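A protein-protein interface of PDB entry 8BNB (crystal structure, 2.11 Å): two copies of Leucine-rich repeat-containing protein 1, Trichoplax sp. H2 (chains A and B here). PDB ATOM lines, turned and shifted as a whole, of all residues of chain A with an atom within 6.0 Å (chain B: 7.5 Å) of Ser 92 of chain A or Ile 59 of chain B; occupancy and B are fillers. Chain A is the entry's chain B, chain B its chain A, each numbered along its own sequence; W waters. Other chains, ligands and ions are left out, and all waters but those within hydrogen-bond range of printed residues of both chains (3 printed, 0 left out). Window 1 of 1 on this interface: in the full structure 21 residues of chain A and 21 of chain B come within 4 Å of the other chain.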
ATOM      1  N   GLY A   4       8.629  14.127  12.872  1.00  0.00           N
ATOM      2  CA  GLY A   4       7.338  13.481  12.733  1.00  0.00           C
ATOM      3  C   GLY A   4       6.314  13.930  13.753  1.00  0.00           C
ATOM      4  O   GLY A   4       6.477  13.691  14.952  1.00  0.00           O
ATOM      5  N   SER A   5       5.252  14.580  13.286  1.00  0.00           N
ATOM      6  CA  SER A   5       4.198  15.053  14.173  1.00  0.00           C
ATOM      7  C   SER A   5       3.227  13.922  14.490  1.00  0.00           C
ATOM      8  O   SER A   5       2.789  13.196  13.591  1.00  0.00           O
ATOM      9  CB  SER A   5       3.449  16.219  13.528  1.00  0.00           C
ATOM     10  OG  SER A   5       4.324  17.297  13.242  1.00  0.00           O
ATOM     11  N   THR A   6       2.894  13.773  15.770  1.00  0.00           N
ATOM     12  CA  THR A   6       1.945  12.761  16.219  1.00  0.00           C
ATOM     13  C   THR A   6       0.550  13.371  16.249  1.00  0.00           C
ATOM     14  O   THR A   6       0.291  14.302  17.021  1.00  0.00           O
ATOM     15  CB  THR A   6       2.330  12.232  17.600  1.00  0.00           C
ATOM     16  OG1 THR A   6       3.649  11.672  17.550  1.00  0.00           O
ATOM     17  CG2 THR A   6       1.345  11.165  18.064  1.00  0.00           C
ATOM     18  N   ILE A   7      -0.346  12.850  15.413  1.00  0.00           N
ATOM     19  CA  ILE A   7      -1.695  13.383  15.256  1.00  0.00           C
ATOM     20  C   ILE A   7      -2.661  12.424  15.940  1.00  0.00           C
ATOM     21  O   ILE A   7      -2.706  11.235  15.606  1.00  0.00           O
ATOM     22  CB  ILE A   7      -2.059  13.560  13.773  1.00  0.00           C
ATOM     23  CG1 ILE A   7      -1.007  14.410  13.049  1.00  0.00           C
ATOM     24  CG2 ILE A   7      -3.441  14.182  13.639  1.00  0.00           C
ATOM     25  CD1 ILE A   7      -0.893  15.832  13.556  1.00  0.00           C
ATOM     26  N   GLY A  57      -1.311  11.058   3.217  1.00  0.00           N
ATOM     27  CA  GLY A  57       0.091  10.814   3.458  1.00  0.00           C
ATOM     28  C   GLY A  57       0.415  10.458   4.893  1.00  0.00           C
ATOM     29  O   GLY A  57       1.489   9.904   5.152  1.00  0.00           O
ATOM     30  N   ASP A  58      -0.480  10.770   5.828  1.00  0.00           N
ATOM     31  CA  ASP A  58      -0.289  10.363   7.210  1.00  0.00           C
ATOM     32  C   ASP A  58      -0.338   8.845   7.311  1.00  0.00           C
ATOM     33  O   ASP A  58      -1.125   8.188   6.625  1.00  0.00           O
ATOM     34  CB  ASP A  58      -1.367  10.979   8.104  1.00  0.00           C
ATOM     35  CG  ASP A  58      -1.264  12.489   8.191  1.00  0.00           C
ATOM     36  OD1 ASP A  58      -0.299  13.057   7.635  1.00  0.00           O
ATOM     37  OD2 ASP A  58      -2.156  13.108   8.811  1.00  0.00           O
ATOM     38  N   ILE A  59       0.511   8.289   8.168  1.00  0.00           N
ATOM     39  CA  ILE A  59       0.527   6.854   8.428  1.00  0.00           C
ATOM     40  C   ILE A  59      -0.352   6.570   9.638  1.00  0.00           C
ATOM     41  O   ILE A  59      -0.199   7.201  10.690  1.00  0.00           O
ATOM     42  CB  ILE A  59       1.961   6.349   8.657  1.00  0.00           C
ATOM     43  CG1 ILE A  59       1.984   4.821   8.712  1.00  0.00           C
ATOM     44  CG2 ILE A  59       2.536   6.922   9.942  1.00  0.00           C
ATOM     45  CD1 ILE A  59       3.373   4.233   8.868  1.00  0.00           C
ATOM     46  N   LEU A  60      -1.277   5.625   9.490  1.00  0.00           N
ATOM     47  CA  LEU A  60      -2.160   5.249  10.586  1.00  0.00           C
ATOM     48  C   LEU A  60      -1.437   4.274  11.506  1.00  0.00           C
ATOM     49  O   LEU A  60      -0.968   3.221  11.060  1.00  0.00           O
ATOM     50  CB  LEU A  60      -3.448   4.625  10.054  1.00  0.00           C
ATOM     51  CG  LEU A  60      -4.362   5.529   9.227  1.00  0.00           C
ATOM     52  CD1 LEU A  60      -5.571   4.749   8.735  1.00  0.00           C
ATOM     53  CD2 LEU A  60      -4.798   6.735  10.042  1.00  0.00           C
ATOM     54  N   LEU A  61      -1.346   4.625  12.785  1.00  0.00           N
ATOM     55  CA  LEU A  61      -0.707   3.778  13.781  1.00  0.00           C
ATOM     56  C   LEU A  61      -1.689   3.109  14.724  1.00  0.00           C
ATOM     57  O   LEU A  61      -1.407   2.010  15.207  1.00  0.00           O
ATOM     58  CB  LEU A  61       0.292   4.593  14.612  1.00  0.00           C
ATOM     59  CG  LEU A  61       1.448   5.228  13.833  1.00  0.00           C
ATOM     60  CD1 LEU A  61       2.329   6.051  14.759  1.00  0.00           C
ATOM     61  CD2 LEU A  61       2.266   4.164  13.121  1.00  0.00           C
ATOM     62  N   VAL A  90      -4.825   7.582  15.773  1.00  0.00           N
ATOM     63  CA  VAL A  90      -3.467   8.037  16.048  1.00  0.00           C
ATOM     64  C   VAL A  90      -2.632   7.751  14.807  1.00  0.00           C
ATOM     65  O   VAL A  90      -2.525   6.595  14.376  1.00  0.00           O
ATOM     66  CB  VAL A  90      -2.862   7.340  17.277  1.00  0.00           C
ATOM     67  CG1 VAL A  90      -1.460   7.882  17.568  1.00  0.00           C
ATOM     68  CG2 VAL A  90      -3.772   7.498  18.483  1.00  0.00           C
ATOM     69  N   ALA A  91      -2.032   8.801  14.248  1.00  0.00           N
ATOM     70  CA  ALA A  91      -1.239   8.715  13.033  1.00  0.00           C
ATOM     71  C   ALA A  91       0.017   9.555  13.202  1.00  0.00           C
ATOM     72  O   ALA A  91       0.177  10.286  14.184  1.00  0.00           O
ATOM     73  CB  ALA A  91      -2.036   9.188  11.810  1.00  0.00           C
ATOM     74  N   SER A  92       0.913   9.457  12.224  1.00  0.00           N
ATOM     75  CA  SER A  92       2.147  10.227  12.223  1.00  0.00           C
ATOM     76  C   SER A  92       2.331  10.885  10.865  1.00  0.00           C
ATOM     77  O   SER A  92       2.102  10.261   9.823  1.00  0.00           O
ATOM     78  CB  SER A  92       3.361   9.349  12.548  1.00  0.00           C
ATOM     79  OG  SER A  92       4.529  10.137  12.706  1.00  0.00           O
ATOM     80  N   ARG A  93       2.737  12.150  10.888  1.00  0.00           N
ATOM     81  CA  ARG A  93       2.954  12.946   9.686  1.00  0.00           C
ATOM     82  C   ARG A  93       4.434  13.286   9.608  1.00  0.00           C
ATOM     83  O   ARG A  93       4.956  13.994  10.475  1.00  0.00           O
ATOM     84  CB  ARG A  93       2.105  14.217   9.717  1.00  0.00           C
ATOM     85  CG  ARG A  93       2.191  15.070   8.463  1.00  0.00           C
ATOM     86  CD  ARG A  93       1.205  16.224   8.540  1.00  0.00           C
ATOM     87  NE  ARG A  93      -0.161  15.744   8.718  1.00  0.00           N
ATOM     88  CZ  ARG A  93      -1.138  16.439   9.284  1.00  0.00           C
ATOM     89  NH1 ARG A  93      -0.942  17.665   9.742  1.00  0.00           N
ATOM     90  NH2 ARG A  93      -2.341  15.885   9.401  1.00  0.00           N
ATOM     91  N   GLN A  94       5.108  12.774   8.585  1.00  0.00           N
ATOM     92  CA  GLN A  94       6.543  12.962   8.443  1.00  0.00           C
ATOM     93  C   GLN A  94       6.834  14.251   7.688  1.00  0.00           C
ATOM     94  O   GLN A  94       6.164  14.576   6.704  1.00  0.00           O
ATOM     95  CB  GLN A  94       7.171  11.777   7.709  1.00  0.00           C
ATOM     96  CG  GLN A  94       8.689  11.850   7.596  1.00  0.00           C
ATOM     97  CD  GLN A  94       9.281  10.630   6.918  1.00  0.00           C
ATOM     98  OE1 GLN A  94       9.710  10.694   5.766  1.00  0.00           O
ATOM     99  NE2 GLN A  94       9.305   9.510   7.631  1.00  0.00           N
ATOM    100  N   SER B   5       7.716   0.343   4.732  1.00  0.00           N
ATOM    101  CA  SER B   5       8.123  -1.014   5.071  1.00  0.00           C
ATOM    102  C   SER B   5       8.165  -1.180   6.583  1.00  0.00           C
ATOM    103  O   SER B   5       8.695  -0.323   7.297  1.00  0.00           O
ATOM    104  CB  SER B   5       9.490  -1.332   4.464  1.00  0.00           C
ATOM    105  OG  SER B   5       9.462  -1.220   3.052  1.00  0.00           O
ATOM    106  N   ILE B   7       9.695  -2.871   9.662  1.00  0.00           N
ATOM    107  CA  ILE B   7      10.972  -3.478  10.013  1.00  0.00           C
ATOM    108  C   ILE B   7      10.863  -4.021  11.430  1.00  0.00           C
ATOM    109  O   ILE B   7      10.535  -3.276  12.360  1.00  0.00           O
ATOM    110  CB  ILE B   7      12.122  -2.463   9.910  1.00  0.00           C
ATOM    111  CG1 ILE B   7      12.165  -1.821   8.518  1.00  0.00           C
ATOM    112  CG2 ILE B   7      13.440  -3.131  10.248  1.00  0.00           C
ATOM    113  CD1 ILE B   7      12.455  -2.790   7.389  1.00  0.00           C
ATOM    114  N   THR B  24      16.392  10.525  17.535  1.00  0.00           N
ATOM    115  CA  THR B  24      15.924  11.895  17.669  1.00  0.00           C
ATOM    116  C   THR B  24      14.401  11.877  17.711  1.00  0.00           C
ATOM    117  O   THR B  24      13.763  10.861  17.426  1.00  0.00           O
ATOM    118  CB  THR B  24      16.426  12.783  16.521  1.00  0.00           C
ATOM    119  OG1 THR B  24      16.015  14.138  16.742  1.00  0.00           O
ATOM    120  CG2 THR B  24      15.875  12.304  15.182  1.00  0.00           C
ATOM    121  N   GLN B  29       4.735  18.482  21.649  1.00  0.00           N
ATOM    122  CA  GLN B  29       4.038  19.315  20.685  1.00  0.00           C
ATOM    123  C   GLN B  29       3.111  20.292  21.401  1.00  0.00           C
ATOM    124  O   GLN B  29       2.747  20.104  22.564  1.00  0.00           O
ATOM    125  CB  GLN B  29       3.240  18.453  19.709  1.00  0.00           C
ATOM    126  CG  GLN B  29       4.085  17.444  18.943  1.00  0.00           C
ATOM    127  CD  GLN B  29       3.268  16.501  18.070  1.00  0.00           C
ATOM    128  OE1 GLN B  29       3.833  15.694  17.330  1.00  0.00           O
ATOM    129  NE2 GLN B  29       1.941  16.588  18.154  1.00  0.00           N
ATOM    130  N   SER B  35       6.197  14.176  19.642  1.00  0.00           N
ATOM    131  CA  SER B  35       6.490  13.858  18.254  1.00  0.00           C
ATOM    132  C   SER B  35       7.075  12.454  18.130  1.00  0.00           C
ATOM    133  O   SER B  35       7.523  11.845  19.104  1.00  0.00           O
ATOM    134  CB  SER B  35       7.466  14.879  17.667  1.00  0.00           C
ATOM    135  OG  SER B  35       8.709  14.854  18.347  1.00  0.00           O
ATOM    136  N   GLY B  36       7.067  11.943  16.902  1.00  0.00           N
ATOM    137  CA  GLY B  36       7.611  10.627  16.650  1.00  0.00           C
ATOM    138  C   GLY B  36       9.104  10.562  16.905  1.00  0.00           C
ATOM    139  O   GLY B  36       9.824  11.559  16.851  1.00  0.00           O
ATOM    140  N   ILE B  37       9.572   9.351  17.193  1.00  0.00           N
ATOM    141  CA  ILE B  37      10.975   9.087  17.493  1.00  0.00           C
ATOM    142  C   ILE B  37      11.578   8.343  16.311  1.00  0.00           C
ATOM    143  O   ILE B  37      11.026   7.332  15.858  1.00  0.00           O
ATOM    144  CB  ILE B  37      11.128   8.288  18.799  1.00  0.00           C
ATOM    145  CG1 ILE B  37      10.465   9.052  19.949  1.00  0.00           C
ATOM    146  CG2 ILE B  37      12.604   8.030  19.101  1.00  0.00           C
ATOM    147  CD1 ILE B  37      10.564   8.372  21.294  1.00  0.00           C
ATOM    148  N   TYR B  38      12.703   8.846  15.811  1.00  0.00           N
ATOM    149  CA  TYR B  38      13.362   8.308  14.632  1.00  0.00           C
ATOM    150  C   TYR B  38      14.780   7.868  14.971  1.00  0.00           C
ATOM    151  O   TYR B  38      15.389   8.344  15.934  1.00  0.00           O
ATOM    152  CB  TYR B  38      13.416   9.348  13.503  1.00  0.00           C
ATOM    153  CG  TYR B  38      12.076   9.706  12.903  1.00  0.00           C
ATOM    154  CD1 TYR B  38      11.181  10.518  13.585  1.00  0.00           C
ATOM    155  CD2 TYR B  38      11.716   9.248  11.642  1.00  0.00           C
ATOM    156  CE1 TYR B  38       9.958  10.853  13.034  1.00  0.00           C
ATOM    157  CE2 TYR B  38      10.497   9.577  11.084  1.00  0.00           C
ATOM    158  CZ  TYR B  38       9.622  10.379  11.783  1.00  0.00           C
ATOM    159  OH  TYR B  38       8.409  10.709  11.226  1.00  0.00           O
ATOM    160  N   ILE B  39      15.302   6.949  14.165  1.00  0.00           N
ATOM    161  CA  ILE B  39      16.724   6.624  14.191  1.00  0.00           C
ATOM    162  C   ILE B  39      17.460   7.710  13.416  1.00  0.00           C
ATOM    163  O   ILE B  39      17.151   7.969  12.249  1.00  0.00           O
ATOM    164  CB  ILE B  39      16.997   5.238  13.591  1.00  0.00           C
ATOM    165  CG1 ILE B  39      16.241   4.160  14.371  1.00  0.00           C
ATOM    166  CG2 ILE B  39      18.500   4.947  13.587  1.00  0.00           C
ATOM    167  CD1 ILE B  39      16.355   2.779  13.768  1.00  0.00           C
ATOM    168  N   LEU B  54      17.982  -2.370  10.438  1.00  0.00           N
ATOM    169  CA  LEU B  54      17.578  -0.998  10.698  1.00  0.00           C
ATOM    170  C   LEU B  54      18.399  -0.025   9.857  1.00  0.00           C
ATOM    171  O   LEU B  54      19.479  -0.349   9.354  1.00  0.00           O
ATOM    172  CB  LEU B  54      17.733  -0.665  12.182  1.00  0.00           C
ATOM    173  CG  LEU B  54      16.793  -1.411  13.131  1.00  0.00           C
ATOM    174  CD1 LEU B  54      17.229  -1.215  14.576  1.00  0.00           C
ATOM    175  CD2 LEU B  54      15.355  -0.950  12.937  1.00  0.00           C
ATOM    176  N   SER B  55      17.874   1.190   9.715  1.00  0.00           N
ATOM    177  CA  SER B  55      18.536   2.223   8.935  1.00  0.00           C
ATOM    178  C   SER B  55      18.150   3.589   9.480  1.00  0.00           C
ATOM    179  O   SER B  55      17.052   3.776  10.010  1.00  0.00           O
ATOM    180  CB  SER B  55      18.169   2.131   7.448  1.00  0.00           C
ATOM    181  OG  SER B  55      18.665   0.937   6.872  1.00  0.00           O
ATOM    182  N   ALA B  56      19.065   4.545   9.332  1.00  0.00           N
ATOM    183  CA  ALA B  56      18.785   5.915   9.732  1.00  0.00           C
ATOM    184  C   ALA B  56      17.588   6.458   8.962  1.00  0.00           C
ATOM    185  O   ALA B  56      17.429   6.201   7.765  1.00  0.00           O
ATOM    186  CB  ALA B  56      20.011   6.796   9.494  1.00  0.00           C
ATOM    187  N   GLY B  57      16.745   7.218   9.657  1.00  0.00           N
ATOM    188  CA  GLY B  57      15.502   7.707   9.112  1.00  0.00           C
ATOM    189  C   GLY B  57      14.288   6.876   9.477  1.00  0.00           C
ATOM    190  O   GLY B  57      13.160   7.366   9.350  1.00  0.00           O
ATOM    191  N   ASP B  58      14.488   5.637   9.921  1.00  0.00           N
ATOM    192  CA  ASP B  58      13.368   4.816  10.361  1.00  0.00           C
ATOM    193  C   ASP B  58      12.716   5.420  11.597  1.00  0.00           C
ATOM    194  O   ASP B  58      13.390   5.965  12.474  1.00  0.00           O
ATOM    195  CB  ASP B  58      13.838   3.392  10.666  1.00  0.00           C
ATOM    196  CG  ASP B  58      14.319   2.659   9.435  1.00  0.00           C
ATOM    197  OD1 ASP B  58      14.221   3.224   8.326  1.00  0.00           O
ATOM    198  OD2 ASP B  58      14.790   1.511   9.577  1.00  0.00           O
ATOM    199  N   ILE B  59      11.392   5.321  11.663  1.00  0.00           N
ATOM    200  CA  ILE B  59      10.640   5.760  12.831  1.00  0.00           C
ATOM    201  C   ILE B  59      10.450   4.562  13.750  1.00  0.00           C
ATOM    202  O   ILE B  59      10.003   3.497  13.313  1.00  0.00           O
ATOM    203  CB  ILE B  59       9.286   6.369  12.424  1.00  0.00           C
ATOM    204  CG1 ILE B  59       8.606   7.007  13.639  1.00  0.00           C
ATOM    205  CG2 ILE B  59       8.379   5.311  11.820  1.00  0.00           C
ATOM    206  CD1 ILE B  59       7.290   7.685  13.319  1.00  0.00           C
ATOM    207  N   LEU B  60      10.804   4.731  15.020  1.00  0.00           N
ATOM    208  CA  LEU B  60      10.671   3.656  15.994  1.00  0.00           C
ATOM    209  C   LEU B  60       9.233   3.604  16.495  1.00  0.00           C
ATOM    210  O   LEU B  60       8.709   4.604  16.997  1.00  0.00           O
ATOM    211  CB  LEU B  60      11.639   3.863  17.155  1.00  0.00           C
ATOM    212  CG  LEU B  60      13.124   3.811  16.789  1.00  0.00           C
ATOM    213  CD1 LEU B  60      13.985   4.068  18.017  1.00  0.00           C
ATOM    214  CD2 LEU B  60      13.485   2.480  16.153  1.00  0.00           C
ATOM    215  N   LEU B  61       8.602   2.439  16.363  1.00  0.00           N
ATOM    216  CA  LEU B  61       7.230   2.247  16.808  1.00  0.00           C
ATOM    217  C   LEU B  61       7.116   1.422  18.079  1.00  0.00           C
ATOM    218  O   LEU B  61       6.188   1.646  18.857  1.00  0.00           O
ATOM    219  CB  LEU B  61       6.407   1.568  15.706  1.00  0.00           C
ATOM    220  CG  LEU B  61       6.309   2.331  14.383  1.00  0.00           C
ATOM    221  CD1 LEU B  61       5.519   1.530  13.361  1.00  0.00           C
ATOM    222  CD2 LEU B  61       5.682   3.703  14.588  1.00  0.00           C
ATOM    223  N   LYS B  62       8.038   0.490  18.317  1.00  0.00           N
ATOM    224  CA  LYS B  62       7.941  -0.379  19.482  1.00  0.00           C
ATOM    225  C   LYS B  62       9.328  -0.867  19.879  1.00  0.00           C
ATOM    226  O   LYS B  62      10.146  -1.192  19.017  1.00  0.00           O
ATOM    227  CB  LYS B  62       7.024  -1.574  19.201  1.00  0.00           C
ATOM    228  CG  LYS B  62       6.222  -2.037  20.404  1.00  0.00           C
ATOM    229  CD  LYS B  62       5.384  -3.262  20.076  1.00  0.00           C
ATOM    230  CE  LYS B  62       4.358  -3.536  21.162  1.00  0.00           C
ATOM    231  NZ  LYS B  62       3.904  -4.955  21.160  1.00  0.00           N
ATOM    232  N   MET B  68       6.437   3.421  21.200  1.00  0.00           N
ATOM    233  CA  MET B  68       7.207   4.655  21.115  1.00  0.00           C
ATOM    234  C   MET B  68       6.401   5.804  20.524  1.00  0.00           C
ATOM    235  O   MET B  68       6.971   6.861  20.232  1.00  0.00           O
ATOM    236  CB  MET B  68       8.472   4.428  20.285  1.00  0.00           C
ATOM    237  CG  MET B  68       9.466   3.454  20.903  1.00  0.00           C
ATOM    238  SD  MET B  68      10.183   4.040  22.453  1.00  0.00           S
ATOM    239  CE  MET B  68       9.057   3.351  23.663  1.00  0.00           C
ATOM    240  N   THR B  69       5.097   5.622  20.332  1.00  0.00           N
ATOM    241  CA  THR B  69       4.246   6.653  19.753  1.00  0.00           C
ATOM    242  C   THR B  69       3.645   7.506  20.862  1.00  0.00           C
ATOM    243  O   THR B  69       3.038   6.980  21.801  1.00  0.00           O
ATOM    244  CB  THR B  69       3.141   6.027  18.901  1.00  0.00           C
ATOM    245  OG1 THR B  69       3.730   5.287  17.825  1.00  0.00           O
ATOM    246  CG2 THR B  69       2.223   7.102  18.333  1.00  0.00           C
ATOM    247  N   ILE B  89      12.945  -4.584  18.212  1.00  0.00           N
ATOM    248  CA  ILE B  89      12.572  -3.259  17.736  1.00  0.00           C
ATOM    249  C   ILE B  89      11.644  -3.403  16.539  1.00  0.00           C
ATOM    250  O   ILE B  89      11.884  -4.223  15.639  1.00  0.00           O
ATOM    251  CB  ILE B  89      13.812  -2.424  17.362  1.00  0.00           C
ATOM    252  CG1 ILE B  89      14.695  -2.203  18.594  1.00  0.00           C
ATOM    253  CG2 ILE B  89      13.388  -1.093  16.748  1.00  0.00           C
ATOM    254  CD1 ILE B  89      16.033  -1.570  18.286  1.00  0.00           C
ATOM    255  N   VAL B  90      10.583  -2.600  16.539  1.00  0.00           N
ATOM    256  CA  VAL B  90       9.638  -2.488  15.436  1.00  0.00           C
ATOM    257  C   VAL B  90       9.651  -1.035  14.981  1.00  0.00           C
ATOM    258  O   VAL B  90       9.383  -0.129  15.781  1.00  0.00           O
ATOM    259  CB  VAL B  90       8.221  -2.918  15.849  1.00  0.00           C
ATOM    260  CG1 VAL B  90       7.276  -2.856  14.657  1.00  0.00           C
ATOM    261  CG2 VAL B  90       8.237  -4.314  16.466  1.00  0.00           C
ATOM    262  N   ALA B  91       9.962  -0.819  13.704  1.00  0.00           N
ATOM    263  CA  ALA B  91      10.069   0.510  13.121  1.00  0.00           C
ATOM    264  C   ALA B  91       9.419   0.507  11.745  1.00  0.00           C
ATOM    265  O   ALA B  91       9.010  -0.535  11.226  1.00  0.00           O
ATOM    266  CB  ALA B  91      11.532   0.957  13.025  1.00  0.00           C
ATOM    267  N   SER B  92       9.325   1.694  11.149  1.00  0.00           N
ATOM    268  CA  SER B  92       8.768   1.852   9.812  1.00  0.00           C
ATOM    269  C   SER B  92       9.693   2.714   8.967  1.00  0.00           C
ATOM    270  O   SER B  92      10.202   3.738   9.432  1.00  0.00           O
ATOM    271  CB  SER B  92       7.373   2.479   9.851  1.00  0.00           C
ATOM    272  OG  SER B  92       6.791   2.472   8.559  1.00  0.00           O
ATOM    273  N   ARG B  93       9.894   2.295   7.720  1.00  0.00           N
ATOM    274  CA  ARG B  93      10.774   2.977   6.778  1.00  0.00           C
ATOM    275  C   ARG B  93       9.931   3.517   5.633  1.00  0.00           C
ATOM    276  O   ARG B  93       9.327   2.741   4.886  1.00  0.00           O
ATOM    277  CB  ARG B  93      11.848   2.021   6.261  1.00  0.00           C
ATOM    278  CG  ARG B  93      12.886   2.653   5.352  1.00  0.00           C
ATOM    279  CD  ARG B  93      13.972   1.649   5.020  1.00  0.00           C
ATOM    280  NE  ARG B  93      14.605   1.136   6.230  1.00  0.00           N
ATOM    281  CZ  ARG B  93      15.214  -0.039   6.324  1.00  0.00           C
ATOM    282  NH1 ARG B  93      15.299  -0.861   5.291  1.00  0.00           N
ATOM    283  NH2 ARG B  93      15.742  -0.403   7.489  1.00  0.00           N
ATOM    284  N   GLN B  94       9.887   4.841   5.501  1.00  0.00           N
ATOM    285  CA  GLN B  94       9.045   5.492   4.505  1.00  0.00           C
ATOM    286  C   GLN B  94       9.778   5.647   3.180  1.00  0.00           C
ATOM    287  O   GLN B  94      10.966   5.982   3.144  1.00  0.00           O
ATOM    288  CB  GLN B  94       8.588   6.864   5.003  1.00  0.00           C
ATOM    289  CG  GLN B  94       7.626   7.572   4.056  1.00  0.00           C
ATOM    290  CD  GLN B  94       7.136   8.900   4.598  1.00  0.00           C
ATOM    291  OE1 GLN B  94       7.555   9.963   4.137  1.00  0.00           O
ATOM    292  NE2 GLN B  94       6.243   8.848   5.581  1.00  0.00           N
HETATM  293  O   HOH W   1       6.187   9.838  10.307  1.00  0.00           O
HETATM  294  O   HOH W   2      10.173  13.924  15.337  1.00  0.00           O
HETATM  295  O   HOH W   3       4.919   9.811  15.419  1.00  0.00           O
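Gly 4 of chain A touches Ser 35 of chain B. Gly 4 of chain A touches Tyr 38 of chain B. CA of Ser 5 of chain A touches OE1 of Gln 29 of chain B (3.2 Å). Ser 35 of chain B touches Thr 6 of chain A. Ser 92 of chain B touches Ile 59 of chain A (OG to CD1, 3.9 Å). CD2 of Leu 61 of chain A touches CD2 of Leu 61 of chain B (3.7 Å). Thr 69 of chain B touches Leu 61 of chain A. CG1 of Val 90 of chain A touches CG2 of Thr 69 of chain B, 3.8 Å away. CD1 of Ile 59 of chain B touches OG of Ser 92 of chain A, at 3.7 Å. Gln 94 of chain A touches Tyr 38 of chain B.
Of the printed residues of chain B, Thr 6 of chain A touches Gln 29 (2.6 Å), Ser 35 (3.6 Å) and Gly 36 (3.5 Å). Of chain B, only Ile 59 comes within 4 Å of Ser 92 of chain A. Printed residues of chain B within 4 Å of Gln 94 of chain A: Tyr 38 and Gln 94. Of the printed residues of chain A, Gly 36 of chain B touches Gly 4 and Thr 6. Of the printed residues of chain A, Tyr 38 of chain B touches Gly 4 (3.3 Å) and Gln 94 (3.7 Å). Of the printed residues of chain A, Ile 59 of chain B touches Ser 92. Printed residues of chain A within 4 Å of Thr 69 of chain B: Leu 61 and Val 90. The nearest residue of chain B that does not touch Ser 92 of chain A is Tyr 38 of chain B (4.2 Å). The nearest printed residue of chain A that does not touch Ser 35 of chain B is Ser 5 of chain A (4.8 Å).
OE1 of Gln 94 of chain B sits close to OE1 of Gln 94 of chain A (2.8 Å). The side-chain amide oxygen (OE1) of Gln 29 of chain B is in hydrogen-bond range of the backbone NH (N) of Thr 6 of chain A, at 2.6 Å. The backbone NH of Gly 36 of chain B is in hydrogen-bond range of the side-chain hydroxyl of Thr 6 of chain A (3.5 Å). The backbone carbonyl oxygen (O) of Gly 4 of chain A is in hydrogen-bond range of the backbone NH (N) of Gly 36 of chain B (2.7 Å).
Water W1 lies within hydrogen-bond range of OH of Tyr 38 of chain B (2.6 Å) and OG of Ser 92 of chain A (2.9 Å). Water W3 lies within hydrogen-bond range of OG of Ser 92 of chain A, OG1 of Thr 6 of chain A and N of Gly 36 of chain B. Water W2 lies within hydrogen-bond range of the backbone carbonyl oxygen (O) of Gly 36 of chain B, the backbone NH (N) of Gly 4 of chain A and the side-chain hydroxyl (OG) of Ser 35 of chain B.
The backbone NH (N) of Ser 5 of chain A lies within hydrogen-bond range of the backbone carbonyl oxygen (O) of Arg 93 of chain A (2.9 Å). O of Leu 61 of chain B lies within hydrogen-bond range of N of Met 68 of chain B. N of Leu 61 of chain A sits at hydrogen-bond distance from O of Val 90 of chain A. The backbone carbonyl oxygen of Val 90 of chain B lies within hydrogen-bond range of the backbone NH of Leu 61 of chain B (2.7 Å). The backbone NH (N) of Tyr 38 of chain B is in hydrogen-bond range of the backbone carbonyl oxygen (O) of Thr 24 of chain B (2.8 Å). The backbone NH (N) of Ser 92 of chain A is in hydrogen-bond range of the backbone carbonyl oxygen (O) of Ile 59 of chain A (2.9 Å).
Of the 26 printed residues of chain B, 9 touch a printed residue of chain A. Among the printed residues, 14 pairs touch across the chains.
Ile 59 of chain A touches Ser 92 of chain B, and with the chains exchanged Ser 92 of chain A touches Ile 59 of chain B. Leu 61 of chain B touches its own counterpart, Leu 61 of chain A. Gln 94 of chain B touches its own counterpart, Gln 94 of chain A. 12 positions are printed for both chains.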
